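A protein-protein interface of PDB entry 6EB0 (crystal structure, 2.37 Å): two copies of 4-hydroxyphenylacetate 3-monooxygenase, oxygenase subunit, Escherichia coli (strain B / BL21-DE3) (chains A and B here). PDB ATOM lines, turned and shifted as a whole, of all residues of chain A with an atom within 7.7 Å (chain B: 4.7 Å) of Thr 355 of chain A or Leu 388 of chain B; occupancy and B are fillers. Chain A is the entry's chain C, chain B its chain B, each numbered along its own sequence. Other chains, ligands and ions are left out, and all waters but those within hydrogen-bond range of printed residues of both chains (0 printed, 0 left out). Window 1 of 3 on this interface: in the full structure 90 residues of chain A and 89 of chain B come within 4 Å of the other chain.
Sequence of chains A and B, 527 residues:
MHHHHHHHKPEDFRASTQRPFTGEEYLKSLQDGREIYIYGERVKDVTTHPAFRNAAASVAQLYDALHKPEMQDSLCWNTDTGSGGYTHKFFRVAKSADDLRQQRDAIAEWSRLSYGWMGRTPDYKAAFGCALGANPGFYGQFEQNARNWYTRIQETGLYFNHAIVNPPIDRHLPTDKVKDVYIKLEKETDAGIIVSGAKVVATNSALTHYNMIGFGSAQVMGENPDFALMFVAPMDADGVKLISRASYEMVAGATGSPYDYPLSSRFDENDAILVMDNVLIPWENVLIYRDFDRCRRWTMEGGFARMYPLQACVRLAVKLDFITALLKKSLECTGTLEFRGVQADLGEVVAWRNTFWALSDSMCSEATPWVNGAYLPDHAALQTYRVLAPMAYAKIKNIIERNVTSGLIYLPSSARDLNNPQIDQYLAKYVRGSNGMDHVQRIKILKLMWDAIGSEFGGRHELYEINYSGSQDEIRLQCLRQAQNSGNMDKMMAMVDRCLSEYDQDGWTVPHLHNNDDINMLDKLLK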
ATOM      1  N   CYS A 313      -6.098  15.807 -24.704  1.00  0.00           N
ATOM      2  CA  CYS A 313      -4.900  14.973 -24.698  1.00  0.00           C
ATOM      3  C   CYS A 313      -4.461  14.574 -26.115  1.00  0.00           C
ATOM      4  O   CYS A 313      -3.266  14.562 -26.414  1.00  0.00           O
ATOM      5  CB  CYS A 313      -5.150  13.730 -23.846  1.00  0.00           C
ATOM      6  SG  CYS A 313      -3.716  12.688 -23.568  1.00  0.00           S
ATOM      7  N   ALA A 317      -1.006  15.509 -28.047  1.00  0.00           N
ATOM      8  CA  ALA A 317      -0.136  14.487 -28.617  1.00  0.00           C
ATOM      9  C   ALA A 317       0.166  14.768 -30.088  1.00  0.00           C
ATOM     10  O   ALA A 317       1.279  14.514 -30.551  1.00  0.00           O
ATOM     11  CB  ALA A 317      -0.766  13.097 -28.447  1.00  0.00           C
ATOM     12  N   LEU A 320       2.675  17.443 -30.150  1.00  0.00           N
ATOM     13  CA  LEU A 320       3.984  16.912 -29.782  1.00  0.00           C
ATOM     14  C   LEU A 320       4.582  16.034 -30.881  1.00  0.00           C
ATOM     15  O   LEU A 320       5.802  16.011 -31.039  1.00  0.00           O
ATOM     16  CB  LEU A 320       3.896  16.153 -28.461  1.00  0.00           C
ATOM     17  CG  LEU A 320       3.544  16.998 -27.240  1.00  0.00           C
ATOM     18  CD1 LEU A 320       3.665  16.182 -25.972  1.00  0.00           C
ATOM     19  CD2 LEU A 320       4.397  18.279 -27.162  1.00  0.00           C
ATOM     20  N   GLU A 348      14.180  12.196 -24.911  1.00  0.00           N
ATOM     21  CA  GLU A 348      13.207  12.514 -23.869  1.00  0.00           C
ATOM     22  C   GLU A 348      11.968  13.192 -24.445  1.00  0.00           C
ATOM     23  O   GLU A 348      10.848  12.893 -24.028  1.00  0.00           O
ATOM     24  CB  GLU A 348      13.824  13.376 -22.770  1.00  0.00           C
ATOM     25  CG  GLU A 348      12.839  13.529 -21.609  1.00  0.00           C
ATOM     26  CD  GLU A 348      13.393  14.239 -20.416  1.00  0.00           C
ATOM     27  OE1 GLU A 348      14.560  13.990 -20.073  1.00  0.00           O
ATOM     28  OE2 GLU A 348      12.645  15.024 -19.800  1.00  0.00           O
ATOM     29  N   VAL A 349      12.142  14.086 -25.420  1.00  0.00           N
ATOM     30  CA  VAL A 349      10.987  14.676 -26.092  1.00  0.00           C
ATOM     31  C   VAL A 349      10.111  13.586 -26.707  1.00  0.00           C
ATOM     32  O   VAL A 349       8.881  13.633 -26.596  1.00  0.00           O
ATOM     33  CB  VAL A 349      11.423  15.708 -27.150  1.00  0.00           C
ATOM     34  CG1 VAL A 349      10.220  16.217 -27.922  1.00  0.00           C
ATOM     35  CG2 VAL A 349      12.184  16.859 -26.525  1.00  0.00           C
ATOM     36  N   VAL A 350      10.734  12.595 -27.359  1.00  0.00           N
ATOM     37  CA  VAL A 350      10.006  11.445 -27.901  1.00  0.00           C
ATOM     38  C   VAL A 350       9.214  10.726 -26.807  1.00  0.00           C
ATOM     39  O   VAL A 350       8.075  10.306 -27.028  1.00  0.00           O
ATOM     40  CB  VAL A 350      10.967  10.469 -28.617  1.00  0.00           C
ATOM     41  CG1 VAL A 350      10.259   9.168 -28.925  1.00  0.00           C
ATOM     42  CG2 VAL A 350      11.531  11.066 -29.880  1.00  0.00           C
ATOM     43  N   ALA A 351       9.825  10.519 -25.634  1.00  0.00           N
ATOM     44  CA  ALA A 351       9.124   9.819 -24.557  1.00  0.00           C
ATOM     45  C   ALA A 351       7.887  10.591 -24.094  1.00  0.00           C
ATOM     46  O   ALA A 351       6.843   9.992 -23.813  1.00  0.00           O
ATOM     47  CB  ALA A 351      10.070   9.551 -23.378  1.00  0.00           C
ATOM     48  N   TRP A 352       7.998  11.918 -23.974  1.00  0.00           N
ATOM     49  CA  TRP A 352       6.836  12.716 -23.597  1.00  0.00           C
ATOM     50  C   TRP A 352       5.756  12.613 -24.655  1.00  0.00           C
ATOM     51  O   TRP A 352       4.571  12.489 -24.337  1.00  0.00           O
ATOM     52  CB  TRP A 352       7.219  14.181 -23.379  1.00  0.00           C
ATOM     53  CG  TRP A 352       8.004  14.411 -22.163  1.00  0.00           C
ATOM     54  CD1 TRP A 352       9.295  14.843 -22.094  1.00  0.00           C
ATOM     55  CD2 TRP A 352       7.573  14.222 -20.810  1.00  0.00           C
ATOM     56  NE1 TRP A 352       9.692  14.936 -20.796  1.00  0.00           N
ATOM     57  CE2 TRP A 352       8.660  14.554 -19.981  1.00  0.00           C
ATOM     58  CE3 TRP A 352       6.377  13.795 -20.220  1.00  0.00           C
ATOM     59  CZ2 TRP A 352       8.592  14.485 -18.602  1.00  0.00           C
ATOM     60  CZ3 TRP A 352       6.308  13.731 -18.848  1.00  0.00           C
ATOM     61  CH2 TRP A 352       7.412  14.072 -18.049  1.00  0.00           C
ATOM     62  N   ARG A 353       6.151  12.676 -25.921  1.00  0.00           N
ATOM     63  CA  ARG A 353       5.203  12.468 -27.003  1.00  0.00           C
ATOM     64  C   ARG A 353       4.523  11.103 -26.878  1.00  0.00           C
ATOM     65  O   ARG A 353       3.296  11.005 -26.964  1.00  0.00           O
ATOM     66  CB  ARG A 353       5.924  12.645 -28.348  1.00  0.00           C
ATOM     67  CG  ARG A 353       5.134  12.276 -29.585  1.00  0.00           C
ATOM     68  CD  ARG A 353       5.299  10.798 -29.916  1.00  0.00           C
ATOM     69  NE  ARG A 353       4.476  10.449 -31.055  1.00  0.00           N
ATOM     70  CZ  ARG A 353       4.135   9.218 -31.393  1.00  0.00           C
ATOM     71  NH1 ARG A 353       4.551   8.193 -30.673  1.00  0.00           N
ATOM     72  NH2 ARG A 353       3.364   9.020 -32.443  1.00  0.00           N
ATOM     73  N   ASN A 354       5.302  10.044 -26.642  1.00  0.00           N
ATOM     74  CA  ASN A 354       4.710   8.727 -26.439  1.00  0.00           C
ATOM     75  C   ASN A 354       3.692   8.739 -25.291  1.00  0.00           C
ATOM     76  O   ASN A 354       2.641   8.095 -25.374  1.00  0.00           O
ATOM     77  CB  ASN A 354       5.792   7.688 -26.143  1.00  0.00           C
ATOM     78  CG  ASN A 354       6.723   7.442 -27.300  1.00  0.00           C
ATOM     79  OD1 ASN A 354       6.420   7.744 -28.452  1.00  0.00           O
ATOM     80  ND2 ASN A 354       7.856   6.855 -27.002  1.00  0.00           N
ATOM     81  N   THR A 355       3.997   9.478 -24.226  1.00  0.00           N
ATOM     82  CA  THR A 355       3.213   9.454 -22.998  1.00  0.00           C
ATOM     83  C   THR A 355       1.762   9.840 -23.242  1.00  0.00           C
ATOM     84  O   THR A 355       0.846   9.172 -22.757  1.00  0.00           O
ATOM     85  CB  THR A 355       3.853  10.393 -21.975  1.00  0.00           C
ATOM     86  OG1 THR A 355       5.164   9.915 -21.658  1.00  0.00           O
ATOM     87  CG2 THR A 355       3.011  10.504 -20.717  1.00  0.00           C
ATOM     88  N   PHE A 356       1.534  10.917 -23.990  1.00  0.00           N
ATOM     89  CA  PHE A 356       0.169  11.379 -24.171  1.00  0.00           C
ATOM     90  C   PHE A 356      -0.619  10.524 -25.149  1.00  0.00           C
ATOM     91  O   PHE A 356      -1.819  10.339 -24.949  1.00  0.00           O
ATOM     92  CB  PHE A 356       0.186  12.857 -24.545  1.00  0.00           C
ATOM     93  CG  PHE A 356       0.716  13.684 -23.442  1.00  0.00           C
ATOM     94  CD1 PHE A 356      -0.077  13.944 -22.325  1.00  0.00           C
ATOM     95  CD2 PHE A 356       2.032  14.103 -23.448  1.00  0.00           C
ATOM     96  CE1 PHE A 356       0.417  14.668 -21.265  1.00  0.00           C
ATOM     97  CE2 PHE A 356       2.538  14.818 -22.394  1.00  0.00           C
ATOM     98  CZ  PHE A 356       1.731  15.103 -21.297  1.00  0.00           C
ATOM     99  N   TRP A 357       0.027   9.951 -26.162  1.00  0.00           N
ATOM    100  CA  TRP A 357      -0.651   8.936 -26.962  1.00  0.00           C
ATOM    101  C   TRP A 357      -1.064   7.746 -26.096  1.00  0.00           C
ATOM    102  O   TRP A 357      -2.187   7.238 -26.214  1.00  0.00           O
ATOM    103  CB  TRP A 357       0.252   8.472 -28.105  1.00  0.00           C
ATOM    104  CG  TRP A 357       0.368   9.476 -29.189  1.00  0.00           C
ATOM    105  CD1 TRP A 357       1.481  10.135 -29.559  1.00  0.00           C
ATOM    106  CD2 TRP A 357      -0.688   9.968 -30.019  1.00  0.00           C
ATOM    107  NE1 TRP A 357       1.203  11.003 -30.577  1.00  0.00           N
ATOM    108  CE2 TRP A 357      -0.124  10.917 -30.884  1.00  0.00           C
ATOM    109  CE3 TRP A 357      -2.052   9.686 -30.119  1.00  0.00           C
ATOM    110  CZ2 TRP A 357      -0.870  11.599 -31.836  1.00  0.00           C
ATOM    111  CZ3 TRP A 357      -2.789  10.349 -31.067  1.00  0.00           C
ATOM    112  CH2 TRP A 357      -2.190  11.309 -31.917  1.00  0.00           C
ATOM    113  N   ALA A 358      -0.165   7.300 -25.212  1.00  0.00           N
ATOM    114  CA  ALA A 358      -0.446   6.155 -24.345  1.00  0.00           C
ATOM    115  C   ALA A 358      -1.581   6.463 -23.372  1.00  0.00           C
ATOM    116  O   ALA A 358      -2.417   5.600 -23.098  1.00  0.00           O
ATOM    117  CB  ALA A 358       0.824   5.756 -23.584  1.00  0.00           C
ATOM    118  N   LEU A 359      -1.605   7.685 -22.826  1.00  0.00           N
ATOM    119  CA  LEU A 359      -2.710   8.104 -21.972  1.00  0.00           C
ATOM    120  C   LEU A 359      -4.038   8.036 -22.721  1.00  0.00           C
ATOM    121  O   LEU A 359      -5.035   7.552 -22.173  1.00  0.00           O
ATOM    122  CB  LEU A 359      -2.466   9.517 -21.429  1.00  0.00           C
ATOM    123  CG  LEU A 359      -1.426   9.614 -20.302  1.00  0.00           C
ATOM    124  CD1 LEU A 359      -1.082  11.050 -19.963  1.00  0.00           C
ATOM    125  CD2 LEU A 359      -1.899   8.874 -19.057  1.00  0.00           C
ATOM    126  N   SER A 360      -4.066   8.513 -23.975  1.00  0.00           N
ATOM    127  CA  SER A 360      -5.293   8.430 -24.756  1.00  0.00           C
ATOM    128  C   SER A 360      -5.664   6.981 -25.057  1.00  0.00           C
ATOM    129  O   SER A 360      -6.851   6.663 -25.135  1.00  0.00           O
ATOM    130  CB  SER A 360      -5.187   9.241 -26.058  1.00  0.00           C
ATOM    131  OG  SER A 360      -4.492   8.548 -27.088  1.00  0.00           O
ATOM    132  N   ASP A 361      -4.673   6.102 -25.239  1.00  0.00           N
ATOM    133  CA  ASP A 361      -4.954   4.676 -25.348  1.00  0.00           C
ATOM    134  C   ASP A 361      -5.703   4.192 -24.121  1.00  0.00           C
ATOM    135  O   ASP A 361      -6.722   3.504 -24.223  1.00  0.00           O
ATOM    136  CB  ASP A 361      -3.652   3.868 -25.481  1.00  0.00           C
ATOM    137  CG  ASP A 361      -2.947   4.076 -26.793  1.00  0.00           C
ATOM    138  OD1 ASP A 361      -3.595   4.459 -27.784  1.00  0.00           O
ATOM    139  OD2 ASP A 361      -1.728   3.810 -26.841  1.00  0.00           O
ATOM    140  N   SER A 362      -5.184   4.533 -22.948  1.00  0.00           N
ATOM    141  CA  SER A 362      -5.755   4.064 -21.702  1.00  0.00           C
ATOM    142  C   SER A 362      -7.130   4.669 -21.462  1.00  0.00           C
ATOM    143  O   SER A 362      -7.996   4.014 -20.879  1.00  0.00           O
ATOM    144  CB  SER A 362      -4.802   4.396 -20.557  1.00  0.00           C
ATOM    145  OG  SER A 362      -5.349   3.993 -19.329  1.00  0.00           O
ATOM    146  N   THR A 384      -4.465  12.466 -15.014  1.00  0.00           N
ATOM    147  CA  THR A 384      -3.026  12.330 -15.217  1.00  0.00           C
ATOM    148  C   THR A 384      -2.546  13.185 -16.379  1.00  0.00           C
ATOM    149  O   THR A 384      -1.511  13.845 -16.280  1.00  0.00           O
ATOM    150  CB  THR A 384      -2.663  10.865 -15.469  1.00  0.00           C
ATOM    151  OG1 THR A 384      -3.210  10.055 -14.433  1.00  0.00           O
ATOM    152  CG2 THR A 384      -1.150  10.671 -15.541  1.00  0.00           C
ATOM    153  N   TYR A 385      -3.277  13.179 -17.492  1.00  0.00           N
ATOM    154  CA  TYR A 385      -2.948  14.082 -18.589  1.00  0.00           C
ATOM    155  C   TYR A 385      -2.886  15.528 -18.097  1.00  0.00           C
ATOM    156  O   TYR A 385      -1.942  16.261 -18.406  1.00  0.00           O
ATOM    157  CB  TYR A 385      -3.963  13.939 -19.732  1.00  0.00           C
ATOM    158  CG  TYR A 385      -4.253  15.258 -20.433  1.00  0.00           C
ATOM    159  CD1 TYR A 385      -3.339  15.826 -21.301  1.00  0.00           C
ATOM    160  CD2 TYR A 385      -5.422  15.949 -20.177  1.00  0.00           C
ATOM    161  CE1 TYR A 385      -3.593  17.033 -21.915  1.00  0.00           C
ATOM    162  CE2 TYR A 385      -5.685  17.157 -20.769  1.00  0.00           C
ATOM    163  CZ  TYR A 385      -4.771  17.705 -21.633  1.00  0.00           C
ATOM    164  OH  TYR A 385      -5.047  18.913 -22.229  1.00  0.00           O
ATOM    165  N   LEU A 388       0.363  16.033 -16.041  1.00  0.00           N
ATOM    166  CA  LEU A 388       1.616  15.866 -16.765  1.00  0.00           C
ATOM    167  C   LEU A 388       1.813  16.895 -17.867  1.00  0.00           C
ATOM    168  O   LEU A 388       2.952  17.301 -18.121  1.00  0.00           O
ATOM    169  CB  LEU A 388       1.709  14.464 -17.346  1.00  0.00           C
ATOM    170  CG  LEU A 388       1.899  13.375 -16.286  1.00  0.00           C
ATOM    171  CD1 LEU A 388       2.236  12.071 -16.958  1.00  0.00           C
ATOM    172  CD2 LEU A 388       2.995  13.766 -15.282  1.00  0.00           C
ATOM    173  N   ALA A 389       0.738  17.336 -18.514  1.00  0.00           N
ATOM    174  CA  ALA A 389       0.892  18.189 -19.691  1.00  0.00           C
ATOM    175  C   ALA A 389       1.684  19.458 -19.398  1.00  0.00           C
ATOM    176  O   ALA A 389       2.589  19.790 -20.178  1.00  0.00           O
ATOM    177  CB  ALA A 389      -0.488  18.507 -20.278  1.00  0.00           C
ATOM    178  N   ALA A 392       5.425  18.471 -19.007  1.00  0.00           N
ATOM    179  CA  ALA A 392       6.036  18.042 -20.260  1.00  0.00           C
ATOM    180  C   ALA A 392       6.244  19.221 -21.204  1.00  0.00           C
ATOM    181  O   ALA A 392       7.307  19.352 -21.814  1.00  0.00           O
ATOM    182  CB  ALA A 392       5.188  16.961 -20.927  1.00  0.00           C
ATOM    183  N   THR B 355       0.305   6.994 -14.127  1.00  0.00           N
ATOM    184  CA  THR B 355       1.033   6.999 -15.393  1.00  0.00           C
ATOM    185  C   THR B 355       1.492   5.598 -15.769  1.00  0.00           C
ATOM    186  O   THR B 355       1.318   5.151 -16.906  1.00  0.00           O
ATOM    187  CB  THR B 355       2.234   7.951 -15.296  1.00  0.00           C
ATOM    188  OG1 THR B 355       1.787   9.281 -15.071  1.00  0.00           O
ATOM    189  CG2 THR B 355       3.064   7.931 -16.548  1.00  0.00           C
ATOM    190  N   PHE B 356       2.069   4.884 -14.820  1.00  0.00           N
ATOM    191  CA  PHE B 356       2.611   3.577 -15.155  1.00  0.00           C
ATOM    192  C   PHE B 356       1.520   2.528 -15.323  1.00  0.00           C
ATOM    193  O   PHE B 356       1.678   1.627 -16.144  1.00  0.00           O
ATOM    194  CB  PHE B 356       3.673   3.198 -14.119  1.00  0.00           C
ATOM    195  CG  PHE B 356       4.844   4.125 -14.164  1.00  0.00           C
ATOM    196  CD1 PHE B 356       5.775   4.027 -15.181  1.00  0.00           C
ATOM    197  CD2 PHE B 356       4.974   5.147 -13.248  1.00  0.00           C
ATOM    198  CE1 PHE B 356       6.835   4.913 -15.255  1.00  0.00           C
ATOM    199  CE2 PHE B 356       6.021   6.026 -13.317  1.00  0.00           C
ATOM    200  CZ  PHE B 356       6.960   5.911 -14.316  1.00  0.00           C
ATOM    201  N   LEU B 359       0.466   3.275 -18.965  1.00  0.00           N
ATOM    202  CA  LEU B 359       1.421   2.710 -19.911  1.00  0.00           C
ATOM    203  C   LEU B 359       1.219   1.203 -20.059  1.00  0.00           C
ATOM    204  O   LEU B 359       1.182   0.679 -21.178  1.00  0.00           O
ATOM    205  CB  LEU B 359       2.849   3.024 -19.466  1.00  0.00           C
ATOM    206  CG  LEU B 359       3.335   4.456 -19.667  1.00  0.00           C
ATOM    207  CD1 LEU B 359       4.672   4.669 -18.966  1.00  0.00           C
ATOM    208  CD2 LEU B 359       3.454   4.791 -21.146  1.00  0.00           C
ATOM    209  N   THR B 384       8.963   4.213 -23.203  1.00  0.00           N
ATOM    210  CA  THR B 384       8.495   5.333 -22.397  1.00  0.00           C
ATOM    211  C   THR B 384       8.542   5.000 -20.911  1.00  0.00           C
ATOM    212  O   THR B 384       8.909   5.847 -20.088  1.00  0.00           O
ATOM    213  CB  THR B 384       7.081   5.717 -22.811  1.00  0.00           C
ATOM    214  OG1 THR B 384       7.031   5.868 -24.227  1.00  0.00           O
ATOM    215  CG2 THR B 384       6.659   7.015 -22.156  1.00  0.00           C
ATOM    216  N   TYR B 385       8.143   3.779 -20.548  1.00  0.00           N
ATOM    217  CA  TYR B 385       8.289   3.355 -19.165  1.00  0.00           C
ATOM    218  C   TYR B 385       9.748   3.486 -18.712  1.00  0.00           C
ATOM    219  O   TYR B 385      10.036   4.059 -17.652  1.00  0.00           O
ATOM    220  CB  TYR B 385       7.765   1.923 -18.985  1.00  0.00           C
ATOM    221  CG  TYR B 385       8.552   1.167 -17.958  1.00  0.00           C
ATOM    222  CD1 TYR B 385       8.417   1.460 -16.610  1.00  0.00           C
ATOM    223  CD2 TYR B 385       9.471   0.201 -18.325  1.00  0.00           C
ATOM    224  CE1 TYR B 385       9.150   0.800 -15.654  1.00  0.00           C
ATOM    225  CE2 TYR B 385      10.218  -0.470 -17.362  1.00  0.00           C
ATOM    226  CZ  TYR B 385      10.054  -0.155 -16.028  1.00  0.00           C
ATOM    227  OH  TYR B 385      10.785  -0.793 -15.053  1.00  0.00           O
ATOM    228  N   ARG B 386      10.686   3.010 -19.534  1.00  0.00           N
ATOM    229  CA  ARG B 386      12.091   3.016 -19.134  1.00  0.00           C
ATOM    230  C   ARG B 386      12.606   4.428 -18.882  1.00  0.00           C
ATOM    231  O   ARG B 386      13.411   4.645 -17.976  1.00  0.00           O
ATOM    232  CB  ARG B 386      12.948   2.348 -20.202  1.00  0.00           C
ATOM    233  CG  ARG B 386      12.763   0.876 -20.370  1.00  0.00           C
ATOM    234  CD  ARG B 386      13.805   0.419 -21.366  1.00  0.00           C
ATOM    235  NE  ARG B 386      13.765  -1.000 -21.677  1.00  0.00           N
ATOM    236  CZ  ARG B 386      14.399  -1.934 -20.976  1.00  0.00           C
ATOM    237  NH1 ARG B 386      15.100  -1.591 -19.904  1.00  0.00           N
ATOM    238  NH2 ARG B 386      14.328  -3.207 -21.344  1.00  0.00           N
ATOM    239  N   VAL B 387      12.166   5.392 -19.685  1.00  0.00           N
ATOM    240  CA  VAL B 387      12.626   6.764 -19.541  1.00  0.00           C
ATOM    241  C   VAL B 387      11.975   7.435 -18.334  1.00  0.00           C
ATOM    242  O   VAL B 387      12.648   8.110 -17.551  1.00  0.00           O
ATOM    243  CB  VAL B 387      12.356   7.543 -20.844  1.00  0.00           C
ATOM    244  CG1 VAL B 387      12.646   9.026 -20.669  1.00  0.00           C
ATOM    245  CG2 VAL B 387      13.153   6.953 -21.982  1.00  0.00           C
ATOM    246  N   LEU B 388      10.668   7.250 -18.151  1.00  0.00           N
ATOM    247  CA  LEU B 388       9.942   7.978 -17.116  1.00  0.00           C
ATOM    248  C   LEU B 388      10.213   7.446 -15.713  1.00  0.00           C
ATOM    249  O   LEU B 388      10.260   8.226 -14.755  1.00  0.00           O
ATOM    250  CB  LEU B 388       8.441   7.929 -17.389  1.00  0.00           C
ATOM    251  CG  LEU B 388       7.917   8.706 -18.597  1.00  0.00           C
ATOM    252  CD1 LEU B 388       6.409   8.781 -18.547  1.00  0.00           C
ATOM    253  CD2 LEU B 388       8.533  10.086 -18.648  1.00  0.00           C
ATOM    254  N   ALA B 389      10.396   6.138 -15.574  1.00  0.00           N
ATOM    255  CA  ALA B 389      10.475   5.532 -14.248  1.00  0.00           C
ATOM    256  C   ALA B 389      11.579   6.126 -13.388  1.00  0.00           C
ATOM    257  O   ALA B 389      11.325   6.390 -12.202  1.00  0.00           O
ATOM    258  CB  ALA B 389      10.625   4.015 -14.393  1.00  0.00           C
ATOM    259  N   PRO B 390      12.794   6.356 -13.894  1.00  0.00           N
ATOM    260  CA  PRO B 390      13.813   7.008 -13.054  1.00  0.00           C
ATOM    261  C   PRO B 390      13.455   8.428 -12.655  1.00  0.00           C
ATOM    262  O   PRO B 390      13.763   8.838 -11.533  1.00  0.00           O
ATOM    263  CB  PRO B 390      15.067   6.949 -13.932  1.00  0.00           C
ATOM    264  CG  PRO B 390      14.813   5.787 -14.833  1.00  0.00           C
ATOM    265  CD  PRO B 390      13.365   5.827 -15.138  1.00  0.00           C
ATOM    266  N   MET B 391      12.838   9.201 -13.551  1.00  0.00           N
ATOM    267  CA  MET B 391      12.389  10.544 -13.197  1.00  0.00           C
ATOM    268  C   MET B 391      11.314  10.511 -12.118  1.00  0.00           C
ATOM    269  O   MET B 391      11.374  11.266 -11.148  1.00  0.00           O
ATOM    270  CB  MET B 391      11.854  11.265 -14.437  1.00  0.00           C
ATOM    271  CG  MET B 391      12.905  11.953 -15.312  1.00  0.00           C
ATOM    272  SD  MET B 391      12.136  12.709 -16.774  1.00  0.00           S
ATOM    273  CE  MET B 391      10.529  13.055 -16.057  1.00  0.00           C
ATOM    274  N   ALA B 392      10.293   9.673 -12.298  1.00  0.00           N
ATOM    275  CA  ALA B 392       9.190   9.626 -11.340  1.00  0.00           C
ATOM    276  C   ALA B 392       9.662   9.150  -9.977  1.00  0.00           C
ATOM    277  O   ALA B 392       9.269   9.710  -8.948  1.00  0.00           O
ATOM    278  CB  ALA B 392       8.065   8.722 -11.859  1.00  0.00           C
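Among the printed residues, merely in contact across the chains: Thr 384 of chain A with Thr 355 of chain B (3.3 Å), Thr 355 of chain A with Thr 384 of chain B (3.3 Å), Leu 388 of chain A with Thr 355 of chain B (3.4 Å), Ala 351 of chain A with Thr 384 of chain B (3.4 Å), Trp 352 of chain A with Met 391 of chain B (3.5 Å), Thr 355 of chain A with Leu 388 of chain B (3.5 Å), Ala 358 of chain A with Leu 359 of chain B (3.7 Å), Ala 351 of chain A with Val 387 of chain B (3.8 Å) and Glu 348 of chain A with Met 391 of chain B (3.8 Å).
Leu 388 of chain B touches just one residue of chain A: Thr 355 (3.5 Å).
Printed residues of chain A within 4 Å of Leu 359 of chain B: Ala 358 (3.7 Å).
Printed residues of chain B within 4 Å of Thr 384 of chain A: Thr 355 (3.3 Å).
Of the printed residues of chain B, Ala 351 of chain A touches Thr 384 (3.4 Å) and Val 387 (3.8 Å).
Of the printed residues of chain A, Thr 384 of chain B touches Ala 351 (3.4 Å), Asn 354 (2.9 Å) and Thr 355 (3.3 Å).
Of the printed residues of chain B, Trp 352 of chain A touches Met 391.
Ala 389 of chain B touches none of the printed residues of chain A.
Leu 359 of chain A touches none of the printed residues of chain B.
The nearest residue of chain A that does not touch Leu 388 of chain B is Trp 352 of chain A (4.2 Å).
The nearest printed residue of chain A that does not touch Val 387 of chain B is Glu 348 of chain A (4.6 Å).
Hydrophobic or aromatic side chains of chain A within 4 Å of the printed part of chain B: Ala 351, Trp 352, Ala 358 and Leu 388.
Among the printed residues, 10 pairs touch across the chains.
Among the printed residues, no Asp or Glu carboxylate lies within 4 Å of a Lys or Arg side-chain nitrogen of the other chain.
Thr 355 of chain A touches Thr 384 of chain B, and with the chains exchanged Thr 384 of chain A touches Thr 355 of chain B.
Thr 355 of chain A touches Leu 388 of chain B, and with the chains exchanged Leu 388 of chain A touches Thr 355 of chain B.
Of the 10 pairs that touch across the chains among the printed residues, 4 have their exchanged pair printed and touching as well.
ND2 of Asn 354 of chain A sits close to OG1 of Thr 384 of chain B (3.1 Å).
OE2 of Glu 348 of chain A lies within hydrogen-bond range of NE1 of Trp 352 of chain A.
The side-chain amide oxygen (OD1) of Asn 354 of chain A sits close to the backbone carbonyl oxygen (O) of Val 350 of chain A (3.4 Å).
The backbone carbonyl oxygen (O) of Ala 351 of chain A lies within hydrogen-bond range of the side-chain hydroxyl (OG1) of Thr 355 of chain A (2.7 Å).
OD1 of Asn 354 of chain A sits at hydrogen-bond distance from NH1 of Arg 353 of chain A, at 2.9 Å.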
